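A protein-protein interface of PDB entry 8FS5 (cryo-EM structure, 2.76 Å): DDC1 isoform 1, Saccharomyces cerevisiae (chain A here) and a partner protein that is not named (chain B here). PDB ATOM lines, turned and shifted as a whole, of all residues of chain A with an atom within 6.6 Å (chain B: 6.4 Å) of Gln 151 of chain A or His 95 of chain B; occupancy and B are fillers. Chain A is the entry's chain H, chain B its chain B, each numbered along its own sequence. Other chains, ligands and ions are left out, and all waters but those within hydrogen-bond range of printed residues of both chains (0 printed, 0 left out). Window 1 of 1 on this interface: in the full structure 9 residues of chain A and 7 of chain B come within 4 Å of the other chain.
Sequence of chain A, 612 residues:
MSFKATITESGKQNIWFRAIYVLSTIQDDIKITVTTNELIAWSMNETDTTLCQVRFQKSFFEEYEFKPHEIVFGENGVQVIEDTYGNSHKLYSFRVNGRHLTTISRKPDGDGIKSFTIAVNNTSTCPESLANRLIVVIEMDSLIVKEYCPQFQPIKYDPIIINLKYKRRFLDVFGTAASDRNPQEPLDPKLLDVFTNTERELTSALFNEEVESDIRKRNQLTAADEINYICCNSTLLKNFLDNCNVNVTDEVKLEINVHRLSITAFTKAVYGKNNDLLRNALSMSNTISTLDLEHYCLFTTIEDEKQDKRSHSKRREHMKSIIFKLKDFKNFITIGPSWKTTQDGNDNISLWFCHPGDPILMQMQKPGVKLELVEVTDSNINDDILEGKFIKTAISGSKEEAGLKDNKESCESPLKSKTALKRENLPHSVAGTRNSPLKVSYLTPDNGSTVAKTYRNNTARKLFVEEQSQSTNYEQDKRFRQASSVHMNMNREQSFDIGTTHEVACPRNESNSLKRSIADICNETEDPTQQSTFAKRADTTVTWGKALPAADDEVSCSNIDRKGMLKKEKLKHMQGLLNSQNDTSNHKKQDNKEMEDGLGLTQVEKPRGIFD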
ATOM      1  N   ASP A  29      29.658 -22.411  21.973  1.00  0.00           N
ATOM      2  CA  ASP A  29      29.024 -22.693  23.257  1.00  0.00           C
ATOM      3  C   ASP A  29      29.818 -21.998  24.356  1.00  0.00           C
ATOM      4  O   ASP A  29      31.005 -22.284  24.546  1.00  0.00           O
ATOM      5  CB  ASP A  29      28.939 -24.198  23.506  1.00  0.00           C
ATOM      6  CG  ASP A  29      27.685 -24.816  22.920  1.00  0.00           C
ATOM      7  OD1 ASP A  29      27.688 -25.146  21.716  1.00  0.00           O
ATOM      8  OD2 ASP A  29      26.694 -24.974  23.664  1.00  0.00           O
ATOM      9  N   ARG A  95      27.205 -25.958  29.899  1.00  0.00           N
ATOM     10  CA  ARG A  95      27.453 -25.410  28.574  1.00  0.00           C
ATOM     11  C   ARG A  95      26.163 -24.859  27.981  1.00  0.00           C
ATOM     12  O   ARG A  95      25.123 -25.522  27.992  1.00  0.00           O
ATOM     13  CB  ARG A  95      28.031 -26.479  27.643  1.00  0.00           C
ATOM     14  CG  ARG A  95      29.347 -26.098  26.990  1.00  0.00           C
ATOM     15  CD  ARG A  95      29.730 -27.026  25.832  1.00  0.00           C
ATOM     16  NE  ARG A  95      29.510 -28.442  26.109  1.00  0.00           N
ATOM     17  CZ  ARG A  95      28.479 -29.147  25.664  1.00  0.00           C
ATOM     18  NH1 ARG A  95      27.538 -28.598  24.912  1.00  0.00           N
ATOM     19  NH2 ARG A  95      28.389 -30.436  25.980  1.00  0.00           N
ATOM     20  N   VAL A  96      26.241 -23.645  27.445  1.00  0.00           N
ATOM     21  CA  VAL A  96      25.080 -22.985  26.857  1.00  0.00           C
ATOM     22  C   VAL A  96      25.501 -22.366  25.530  1.00  0.00           C
ATOM     23  O   VAL A  96      26.631 -21.892  25.383  1.00  0.00           O
ATOM     24  CB  VAL A  96      24.480 -21.936  27.825  1.00  0.00           C
ATOM     25  CG1 VAL A  96      25.490 -20.840  28.140  1.00  0.00           C
ATOM     26  CG2 VAL A  96      23.187 -21.351  27.269  1.00  0.00           C
ATOM     27  N   ASN A  97      24.595 -22.405  24.553  1.00  0.00           N
ATOM     28  CA  ASN A  97      24.884 -21.856  23.234  1.00  0.00           C
ATOM     29  C   ASN A  97      25.103 -20.350  23.320  1.00  0.00           C
ATOM     30  O   ASN A  97      24.284 -19.621  23.886  1.00  0.00           O
ATOM     31  CB  ASN A  97      23.739 -22.173  22.272  1.00  0.00           C
ATOM     32  CG  ASN A  97      24.119 -21.962  20.817  1.00  0.00           C
ATOM     33  OD1 ASN A  97      25.204 -21.469  20.507  1.00  0.00           O
ATOM     34  ND2 ASN A  97      23.220 -22.333  19.912  1.00  0.00           N
ATOM     35  N   ARG A  99      25.311 -18.056  20.738  1.00  0.00           N
ATOM     36  CA  ARG A  99      24.422 -17.298  19.868  1.00  0.00           C
ATOM     37  C   ARG A  99      23.007 -17.218  20.422  1.00  0.00           C
ATOM     38  O   ARG A  99      22.265 -16.297  20.067  1.00  0.00           O
ATOM     39  CB  ARG A  99      24.400 -17.916  18.470  1.00  0.00           C
ATOM     40  CG  ARG A  99      25.464 -17.367  17.532  1.00  0.00           C
ATOM     41  CD  ARG A  99      25.492 -18.049  16.159  1.00  0.00           C
ATOM     42  NE  ARG A  99      25.389 -19.505  16.208  1.00  0.00           N
ATOM     43  CZ  ARG A  99      24.259 -20.189  16.079  1.00  0.00           C
ATOM     44  NH1 ARG A  99      23.101 -19.579  15.879  1.00  0.00           N
ATOM     45  NH2 ARG A  99      24.292 -21.516  16.152  1.00  0.00           N
ATOM     46  N   HIS A 100      22.619 -18.163  21.276  1.00  0.00           N
ATOM     47  CA  HIS A 100      21.311 -18.135  21.916  1.00  0.00           C
ATOM     48  C   HIS A 100      21.287 -17.222  23.136  1.00  0.00           C
ATOM     49  O   HIS A 100      20.306 -16.502  23.350  1.00  0.00           O
ATOM     50  CB  HIS A 100      20.897 -19.553  22.313  1.00  0.00           C
ATOM     51  CG  HIS A 100      20.560 -20.431  21.147  1.00  0.00           C
ATOM     52  ND1 HIS A 100      20.143 -21.736  21.295  1.00  0.00           N
ATOM     53  CD2 HIS A 100      20.576 -20.189  19.815  1.00  0.00           C
ATOM     54  CE1 HIS A 100      19.918 -22.260  20.104  1.00  0.00           C
ATOM     55  NE2 HIS A 100      20.174 -21.342  19.189  1.00  0.00           N
ATOM     56  N   ALA A 131      14.452 -28.987  33.707  1.00  0.00           N
ATOM     57  CA  ALA A 131      15.448 -30.059  33.718  1.00  0.00           C
ATOM     58  C   ALA A 131      16.425 -29.826  32.574  1.00  0.00           C
ATOM     59  O   ALA A 131      16.049 -29.875  31.400  1.00  0.00           O
ATOM     60  CB  ALA A 131      14.772 -31.420  33.605  1.00  0.00           C
ATOM     61  N   ASN A 132      17.688 -29.566  32.922  1.00  0.00           N
ATOM     62  CA  ASN A 132      18.766 -29.282  31.973  1.00  0.00           C
ATOM     63  C   ASN A 132      18.455 -28.092  31.071  1.00  0.00           C
ATOM     64  O   ASN A 132      19.017 -27.976  29.977  1.00  0.00           O
ATOM     65  CB  ASN A 132      19.109 -30.513  31.125  1.00  0.00           C
ATOM     66  CG  ASN A 132      20.034 -31.474  31.841  1.00  0.00           C
ATOM     67  OD1 ASN A 132      21.034 -31.066  32.433  1.00  0.00           O
ATOM     68  ND2 ASN A 132      19.708 -32.758  31.790  1.00  0.00           N
ATOM     69  N   ARG A 133      17.570 -27.201  31.510  1.00  0.00           N
ATOM     70  CA  ARG A 133      17.236 -25.989  30.777  1.00  0.00           C
ATOM     71  C   ARG A 133      17.395 -24.790  31.701  1.00  0.00           C
ATOM     72  O   ARG A 133      16.793 -24.746  32.780  1.00  0.00           O
ATOM     73  CB  ARG A 133      15.814 -26.060  30.215  1.00  0.00           C
ATOM     74  CG  ARG A 133      15.727 -26.809  28.894  1.00  0.00           C
ATOM     75  CD  ARG A 133      14.577 -26.299  28.037  1.00  0.00           C
ATOM     76  NE  ARG A 133      13.778 -27.382  27.474  1.00  0.00           N
ATOM     77  CZ  ARG A 133      12.966 -28.168  28.171  1.00  0.00           C
ATOM     78  NH1 ARG A 133      12.806 -28.017  29.475  1.00  0.00           N
ATOM     79  NH2 ARG A 133      12.295 -29.127  27.541  1.00  0.00           N
ATOM     80  N   LEU A 134      18.208 -23.828  31.275  1.00  0.00           N
ATOM     81  CA  LEU A 134      18.525 -22.657  32.080  1.00  0.00           C
ATOM     82  C   LEU A 134      17.318 -21.731  32.146  1.00  0.00           C
ATOM     83  O   LEU A 134      16.512 -21.676  31.214  1.00  0.00           O
ATOM     84  CB  LEU A 134      19.734 -21.927  31.493  1.00  0.00           C
ATOM     85  CG  LEU A 134      20.462 -20.901  32.358  1.00  0.00           C
ATOM     86  CD1 LEU A 134      20.884 -21.522  33.678  1.00  0.00           C
ATOM     87  CD2 LEU A 134      21.673 -20.365  31.613  1.00  0.00           C
ATOM     88  N   CYS A 149      13.875 -20.318  28.087  1.00  0.00           N
ATOM     89  CA  CYS A 149      14.336 -21.591  28.636  1.00  0.00           C
ATOM     90  C   CYS A 149      15.442 -22.187  27.767  1.00  0.00           C
ATOM     91  O   CYS A 149      15.223 -23.180  27.063  1.00  0.00           O
ATOM     92  CB  CYS A 149      13.170 -22.567  28.769  1.00  0.00           C
ATOM     93  SG  CYS A 149      12.068 -22.237  30.163  1.00  0.00           S
ATOM     94  N   PRO A 150      16.641 -21.602  27.786  1.00  0.00           N
ATOM     95  CA  PRO A 150      17.741 -22.178  27.002  1.00  0.00           C
ATOM     96  C   PRO A 150      18.235 -23.483  27.608  1.00  0.00           C
ATOM     97  O   PRO A 150      18.434 -23.592  28.820  1.00  0.00           O
ATOM     98  CB  PRO A 150      18.819 -21.088  27.051  1.00  0.00           C
ATOM     99  CG  PRO A 150      18.522 -20.331  28.295  1.00  0.00           C
ATOM    100  CD  PRO A 150      17.029 -20.324  28.408  1.00  0.00           C
ATOM    101  N   GLN A 151      18.430 -24.478  26.748  1.00  0.00           N
ATOM    102  CA  GLN A 151      18.949 -25.768  27.179  1.00  0.00           C
ATOM    103  C   GLN A 151      20.438 -25.677  27.503  1.00  0.00           C
ATOM    104  O   GLN A 151      21.198 -24.986  26.820  1.00  0.00           O
ATOM    105  CB  GLN A 151      18.692 -26.814  26.091  1.00  0.00           C
ATOM    106  CG  GLN A 151      19.279 -26.451  24.731  1.00  0.00           C
ATOM    107  CD  GLN A 151      19.471 -27.653  23.828  1.00  0.00           C
ATOM    108  OE1 GLN A 151      20.597 -28.082  23.581  1.00  0.00           O
ATOM    109  NE2 GLN A 151      18.369 -28.215  23.349  1.00  0.00           N
ATOM    110  N   PHE A 152      20.853 -26.376  28.560  1.00  0.00           N
ATOM    111  CA  PHE A 152      22.252 -26.405  28.966  1.00  0.00           C
ATOM    112  C   PHE A 152      22.707 -27.844  29.176  1.00  0.00           C
ATOM    113  O   PHE A 152      21.899 -28.755  29.372  1.00  0.00           O
ATOM    114  CB  PHE A 152      22.505 -25.548  30.231  1.00  0.00           C
ATOM    115  CG  PHE A 152      21.917 -26.109  31.507  1.00  0.00           C
ATOM    116  CD1 PHE A 152      22.577 -27.089  32.233  1.00  0.00           C
ATOM    117  CD2 PHE A 152      20.720 -25.621  31.998  1.00  0.00           C
ATOM    118  CE1 PHE A 152      22.043 -27.587  33.404  1.00  0.00           C
ATOM    119  CE2 PHE A 152      20.180 -26.115  33.172  1.00  0.00           C
ATOM    120  CZ  PHE A 152      20.843 -27.098  33.875  1.00  0.00           C
ATOM    121  N   GLN A 153      24.022 -28.032  29.129  1.00  0.00           N
ATOM    122  CA  GLN A 153      24.642 -29.352  29.257  1.00  0.00           C
ATOM    123  C   GLN A 153      25.664 -29.341  30.384  1.00  0.00           C
ATOM    124  O   GLN A 153      26.650 -28.578  30.310  1.00  0.00           O
ATOM    125  CB  GLN A 153      25.305 -29.764  27.946  1.00  0.00           C
ATOM    126  CG  GLN A 153      24.327 -30.131  26.854  1.00  0.00           C
ATOM    127  CD  GLN A 153      24.002 -28.960  25.952  1.00  0.00           C
ATOM    128  OE1 GLN A 153      24.872 -28.159  25.613  1.00  0.00           O
ATOM    129  NE2 GLN A 153      22.740 -28.850  25.563  1.00  0.00           N
ATOM    130  N   VAL B  89      20.891 -29.195   9.506  1.00  0.00           N
ATOM    131  CA  VAL B  89      21.711 -30.260  10.072  1.00  0.00           C
ATOM    132  C   VAL B  89      22.695 -29.659  11.067  1.00  0.00           C
ATOM    133  O   VAL B  89      22.921 -30.212  12.148  1.00  0.00           O
ATOM    134  CB  VAL B  89      22.447 -31.041   8.967  1.00  0.00           C
ATOM    135  CG1 VAL B  89      23.327 -32.127   9.573  1.00  0.00           C
ATOM    136  CG2 VAL B  89      21.452 -31.636   7.984  1.00  0.00           C
ATOM    137  N   ARG B  90      23.276 -28.516  10.712  1.00  0.00           N
ATOM    138  CA  ARG B  90      24.277 -27.861  11.540  1.00  0.00           C
ATOM    139  C   ARG B  90      23.688 -27.166  12.762  1.00  0.00           C
ATOM    140  O   ARG B  90      24.414 -26.948  13.738  1.00  0.00           O
ATOM    141  CB  ARG B  90      25.068 -26.847  10.707  1.00  0.00           C
ATOM    142  CG  ARG B  90      26.294 -27.430  10.023  1.00  0.00           C
ATOM    143  CD  ARG B  90      27.246 -26.338   9.563  1.00  0.00           C
ATOM    144  NE  ARG B  90      26.539 -25.227   8.934  1.00  0.00           N
ATOM    145  CZ  ARG B  90      26.850 -24.716   7.752  1.00  0.00           C
ATOM    146  NH1 ARG B  90      27.858 -25.190   7.037  1.00  0.00           N
ATOM    147  NH2 ARG B  90      26.133 -23.703   7.273  1.00  0.00           N
ATOM    148  N   ASN B  91      22.406 -26.803  12.735  1.00  0.00           N
ATOM    149  CA  ASN B  91      21.821 -26.115  13.879  1.00  0.00           C
ATOM    150  C   ASN B  91      20.768 -26.958  14.586  1.00  0.00           C
ATOM    151  O   ASN B  91      20.934 -27.293  15.762  1.00  0.00           O
ATOM    152  CB  ASN B  91      21.207 -24.785  13.437  1.00  0.00           C
ATOM    153  CG  ASN B  91      22.250 -23.713  13.202  1.00  0.00           C
ATOM    154  OD1 ASN B  91      23.315 -23.720  13.818  1.00  0.00           O
ATOM    155  ND2 ASN B  91      21.949 -22.781  12.304  1.00  0.00           N
ATOM    156  N   GLN B  92      19.702 -27.344  13.878  1.00  0.00           N
ATOM    157  CA  GLN B  92      18.595 -28.033  14.539  1.00  0.00           C
ATOM    158  C   GLN B  92      18.995 -29.432  14.987  1.00  0.00           C
ATOM    159  O   GLN B  92      18.780 -29.806  16.149  1.00  0.00           O
ATOM    160  CB  GLN B  92      17.383 -28.094  13.610  1.00  0.00           C
ATOM    161  CG  GLN B  92      16.173 -28.783  14.223  1.00  0.00           C
ATOM    162  CD  GLN B  92      14.964 -28.765  13.308  1.00  0.00           C
ATOM    163  OE1 GLN B  92      15.072 -28.460  12.122  1.00  0.00           O
ATOM    164  NE2 GLN B  92      13.801 -29.093  13.860  1.00  0.00           N
ATOM    165  N   ILE B  93      19.591 -30.213  14.089  1.00  0.00           N
ATOM    166  CA  ILE B  93      20.032 -31.557  14.440  1.00  0.00           C
ATOM    167  C   ILE B  93      21.162 -31.522  15.464  1.00  0.00           C
ATOM    168  O   ILE B  93      21.200 -32.361  16.369  1.00  0.00           O
ATOM    169  CB  ILE B  93      20.447 -32.325  13.173  1.00  0.00           C
ATOM    170  CG1 ILE B  93      19.293 -32.352  12.169  1.00  0.00           C
ATOM    171  CG2 ILE B  93      20.868 -33.746  13.518  1.00  0.00           C
ATOM    172  CD1 ILE B  93      19.561 -33.206  10.948  1.00  0.00           C
ATOM    173  N   LYS B  94      22.074 -30.553  15.352  1.00  0.00           N
ATOM    174  CA  LYS B  94      23.156 -30.432  16.325  1.00  0.00           C
ATOM    175  C   LYS B  94      22.621 -30.106  17.716  1.00  0.00           C
ATOM    176  O   LYS B  94      23.092 -30.665  18.712  1.00  0.00           O
ATOM    177  CB  LYS B  94      24.154 -29.370  15.867  1.00  0.00           C
ATOM    178  CG  LYS B  94      25.211 -29.015  16.900  1.00  0.00           C
ATOM    179  CD  LYS B  94      26.562 -28.776  16.247  1.00  0.00           C
ATOM    180  CE  LYS B  94      27.350 -27.708  16.986  1.00  0.00           C
ATOM    181  NZ  LYS B  94      26.598 -26.425  17.076  1.00  0.00           N
ATOM    182  N   HIS B  95      21.633 -29.209  17.807  1.00  0.00           N
ATOM    183  CA  HIS B  95      21.067 -28.871  19.108  1.00  0.00           C
ATOM    184  C   HIS B  95      20.247 -30.023  19.674  1.00  0.00           C
ATOM    185  O   HIS B  95      20.232 -30.237  20.892  1.00  0.00           O
ATOM    186  CB  HIS B  95      20.216 -27.606  19.001  1.00  0.00           C
ATOM    187  CG  HIS B  95      20.995 -26.385  18.622  1.00  0.00           C
ATOM    188  ND1 HIS B  95      22.365 -26.306  18.752  1.00  0.00           N
ATOM    189  CD2 HIS B  95      20.597 -25.195  18.112  1.00  0.00           C
ATOM    190  CE1 HIS B  95      22.777 -25.121  18.339  1.00  0.00           C
ATOM    191  NE2 HIS B  95      21.724 -24.427  17.946  1.00  0.00           N
ATOM    192  N   PHE B  96      19.549 -30.769  18.813  1.00  0.00           N
ATOM    193  CA  PHE B  96      18.815 -31.936  19.295  1.00  0.00           C
ATOM    194  C   PHE B  96      19.766 -33.011  19.806  1.00  0.00           C
ATOM    195  O   PHE B  96      19.492 -33.660  20.822  1.00  0.00           O
ATOM    196  CB  PHE B  96      17.917 -32.493  18.191  1.00  0.00           C
ATOM    197  CG  PHE B  96      17.140 -33.711  18.602  1.00  0.00           C
ATOM    198  CD1 PHE B  96      16.004 -33.591  19.386  1.00  0.00           C
ATOM    199  CD2 PHE B  96      17.544 -34.976  18.208  1.00  0.00           C
ATOM    200  CE1 PHE B  96      15.287 -34.707  19.769  1.00  0.00           C
ATOM    201  CE2 PHE B  96      16.831 -36.097  18.589  1.00  0.00           C
ATOM    202  CZ  PHE B  96      15.701 -35.962  19.369  1.00  0.00           C
ATOM    203  N   ALA B  97      20.886 -33.219  19.108  1.00  0.00           N
ATOM    204  CA  ALA B  97      21.879 -34.188  19.558  1.00  0.00           C
ATOM    205  C   ALA B  97      22.547 -33.738  20.852  1.00  0.00           C
ATOM    206  O   ALA B  97      22.817 -34.559  21.735  1.00  0.00           O
ATOM    207  CB  ALA B  97      22.922 -34.408  18.463  1.00  0.00           C
ATOM    208  N   GLN B  98      22.825 -32.439  20.976  1.00  0.00           N
ATOM    209  CA  GLN B  98      23.476 -31.927  22.177  1.00  0.00           C
ATOM    210  C   GLN B  98      22.538 -31.930  23.376  1.00  0.00           C
ATOM    211  O   GLN B  98      23.002 -31.858  24.520  1.00  0.00           O
ATOM    212  CB  GLN B  98      24.001 -30.514  21.925  1.00  0.00           C
ATOM    213  CG  GLN B  98      25.478 -30.447  21.580  1.00  0.00           C
ATOM    214  CD  GLN B  98      25.914 -29.053  21.174  1.00  0.00           C
ATOM    215  OE1 GLN B  98      25.156 -28.091  21.301  1.00  0.00           O
ATOM    216  NE2 GLN B  98      27.141 -28.936  20.681  1.00  0.00           N
ATOM    217  N   LYS B  99      21.229 -32.006  23.139  1.00  0.00           N
ATOM    218  CA  LYS B  99      20.261 -31.968  24.227  1.00  0.00           C
ATOM    219  C   LYS B  99      20.427 -33.178  25.138  1.00  0.00           C
ATOM    220  O   LYS B  99      20.584 -34.314  24.679  1.00  0.00           O
ATOM    221  CB  LYS B  99      18.837 -31.919  23.668  1.00  0.00           C
ATOM    222  CG  LYS B  99      17.760 -31.720  24.721  1.00  0.00           C
ATOM    223  CD  LYS B  99      16.380 -31.649  24.091  1.00  0.00           C
ATOM    224  CE  LYS B  99      16.041 -32.935  23.355  1.00  0.00           C
ATOM    225  NZ  LYS B  99      14.700 -32.869  22.714  1.00  0.00           N
ATOM    226  N   LYS B 100      20.389 -32.926  26.444  1.00  0.00           N
ATOM    227  CA  LYS B 100      20.549 -33.960  27.462  1.00  0.00           C
ATOM    228  C   LYS B 100      19.172 -34.304  28.015  1.00  0.00           C
ATOM    229  O   LYS B 100      18.543 -33.478  28.684  1.00  0.00           O
ATOM    230  CB  LYS B 100      21.486 -33.494  28.575  1.00  0.00           C
ATOM    231  CG  LYS B 100      22.906 -34.026  28.458  1.00  0.00           C
ATOM    232  CD  LYS B 100      23.595 -34.083  29.814  1.00  0.00           C
ATOM    233  CE  LYS B 100      22.727 -34.769  30.860  1.00  0.00           C
ATOM    234  NZ  LYS B 100      22.315 -36.138  30.442  1.00  0.00           N
ATOM    235  N   LYS B 109      18.058 -41.215  22.140  1.00  0.00           N
ATOM    236  CA  LYS B 109      17.267 -40.352  21.275  1.00  0.00           C
ATOM    237  C   LYS B 109      17.346 -40.849  19.838  1.00  0.00           C
ATOM    238  O   LYS B 109      18.335 -41.459  19.423  1.00  0.00           O
ATOM    239  CB  LYS B 109      17.755 -38.905  21.363  1.00  0.00           C
ATOM    240  CG  LYS B 109      17.436 -38.228  22.687  1.00  0.00           C
ATOM    241  CD  LYS B 109      18.087 -36.857  22.781  1.00  0.00           C
ATOM    242  CE  LYS B 109      19.584 -36.937  22.520  1.00  0.00           C
ATOM    243  NZ  LYS B 109      20.228 -35.595  22.552  1.00  0.00           N
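OD1 of Asn 91 of chain B sits at hydrogen-bond distance from NH2 of Arg 99 of chain A, at 3.4 Å.
A ring nitrogen (NE2) of His 95 of chain B lies close to the side-chain amide nitrogen (ND2) of Asn 97 of chain A (3.2 Å).
The side-chain amide oxygen of Gln 151 of chain A sits close to the backbone carbonyl oxygen of His 95 of chain B (3.5 Å).
O of Gln 98 of chain B sits close to NE2 of Gln 153 of chain A.
O of Lys 100 of chain B is in hydrogen-bond range of ND2 of Asn 132 of chain A.
The backbone carbonyl oxygen of Lys 99 of chain B is in hydrogen-bond range of the side-chain amino group of Lys 109 of chain B (2.5 Å).
The guanidinium group (NH1) of Arg 95 of chain A lies within salt-bridge range of the side-chain carboxylate (OD2) of Asp 29 of chain A.
The backbone NH (N) of Arg 95 of chain A lies within hydrogen-bond range of the backbone carbonyl oxygen (O) of Gln 153 of chain A.
The side-chain amide oxygen of Asn 97 of chain A sits at hydrogen-bond distance from the backbone NH of Arg 99 of chain A (3.4 Å).
The side-chain amide nitrogen of Asn 97 of chain A lies within hydrogen-bond range of a ring nitrogen (NE2) of His 100 of chain A, 3.3 Å away.
The side-chain amide oxygen of Gln 151 of chain A lies within hydrogen-bond range of the side-chain amide nitrogen of Gln 153 of chain A (3.0 Å).
Among the printed residues, merely in contact across the chains: Asp 29 of chain A with Gln 98 of chain B, His 100 of chain A with His 95 of chain B and Gln 151 of chain A with Lys 99 of chain B.
Gln 151 of chain A touches just these residues of chain B: His 95 (3.5 Å) and Lys 99 (3.7 Å).
Of chain A, only Asn 97 (3.2 Å), His 100 (3.6 Å) and Gln 151 (3.5 Å) come within 4 Å of His 95 of chain B.
Printed residues of chain A within 4 Å of Lys 100 of chain B: Asn 132 (3.4 Å).
Of the printed residues of chain B, Asn 132 of chain A touches Lys 100 (3.4 Å).
Of the printed residues of chain B, His 100 of chain A touches His 95 (3.6 Å).
Of the printed residues of chain B, Asn 97 of chain A touches His 95.
Printed residues of chain B within 4 Å of Asp 29 of chain A: Gln 98 (3.9 Å).
The nearest residue of chain B that does not touch Gln 151 of chain A is Gln 98 of chain B (4.3 Å).
The nearest printed residue of chain A that does not touch Asn 91 of chain B is Asn 97 of chain A (6.3 Å).
Along chain B the printed residues that touch a printed residue of chain A span positions 91 to 100.
Of the 15 printed residues of chain A, 7 touch a printed residue of chain B.
Hydrophobic or aromatic side chains of chain A that line the printed part of chain B: His 100.
Among the printed residues, no Asp or Glu carboxylate lies within 4 Å of a Lys or Arg side-chain nitrogen of the other chain.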
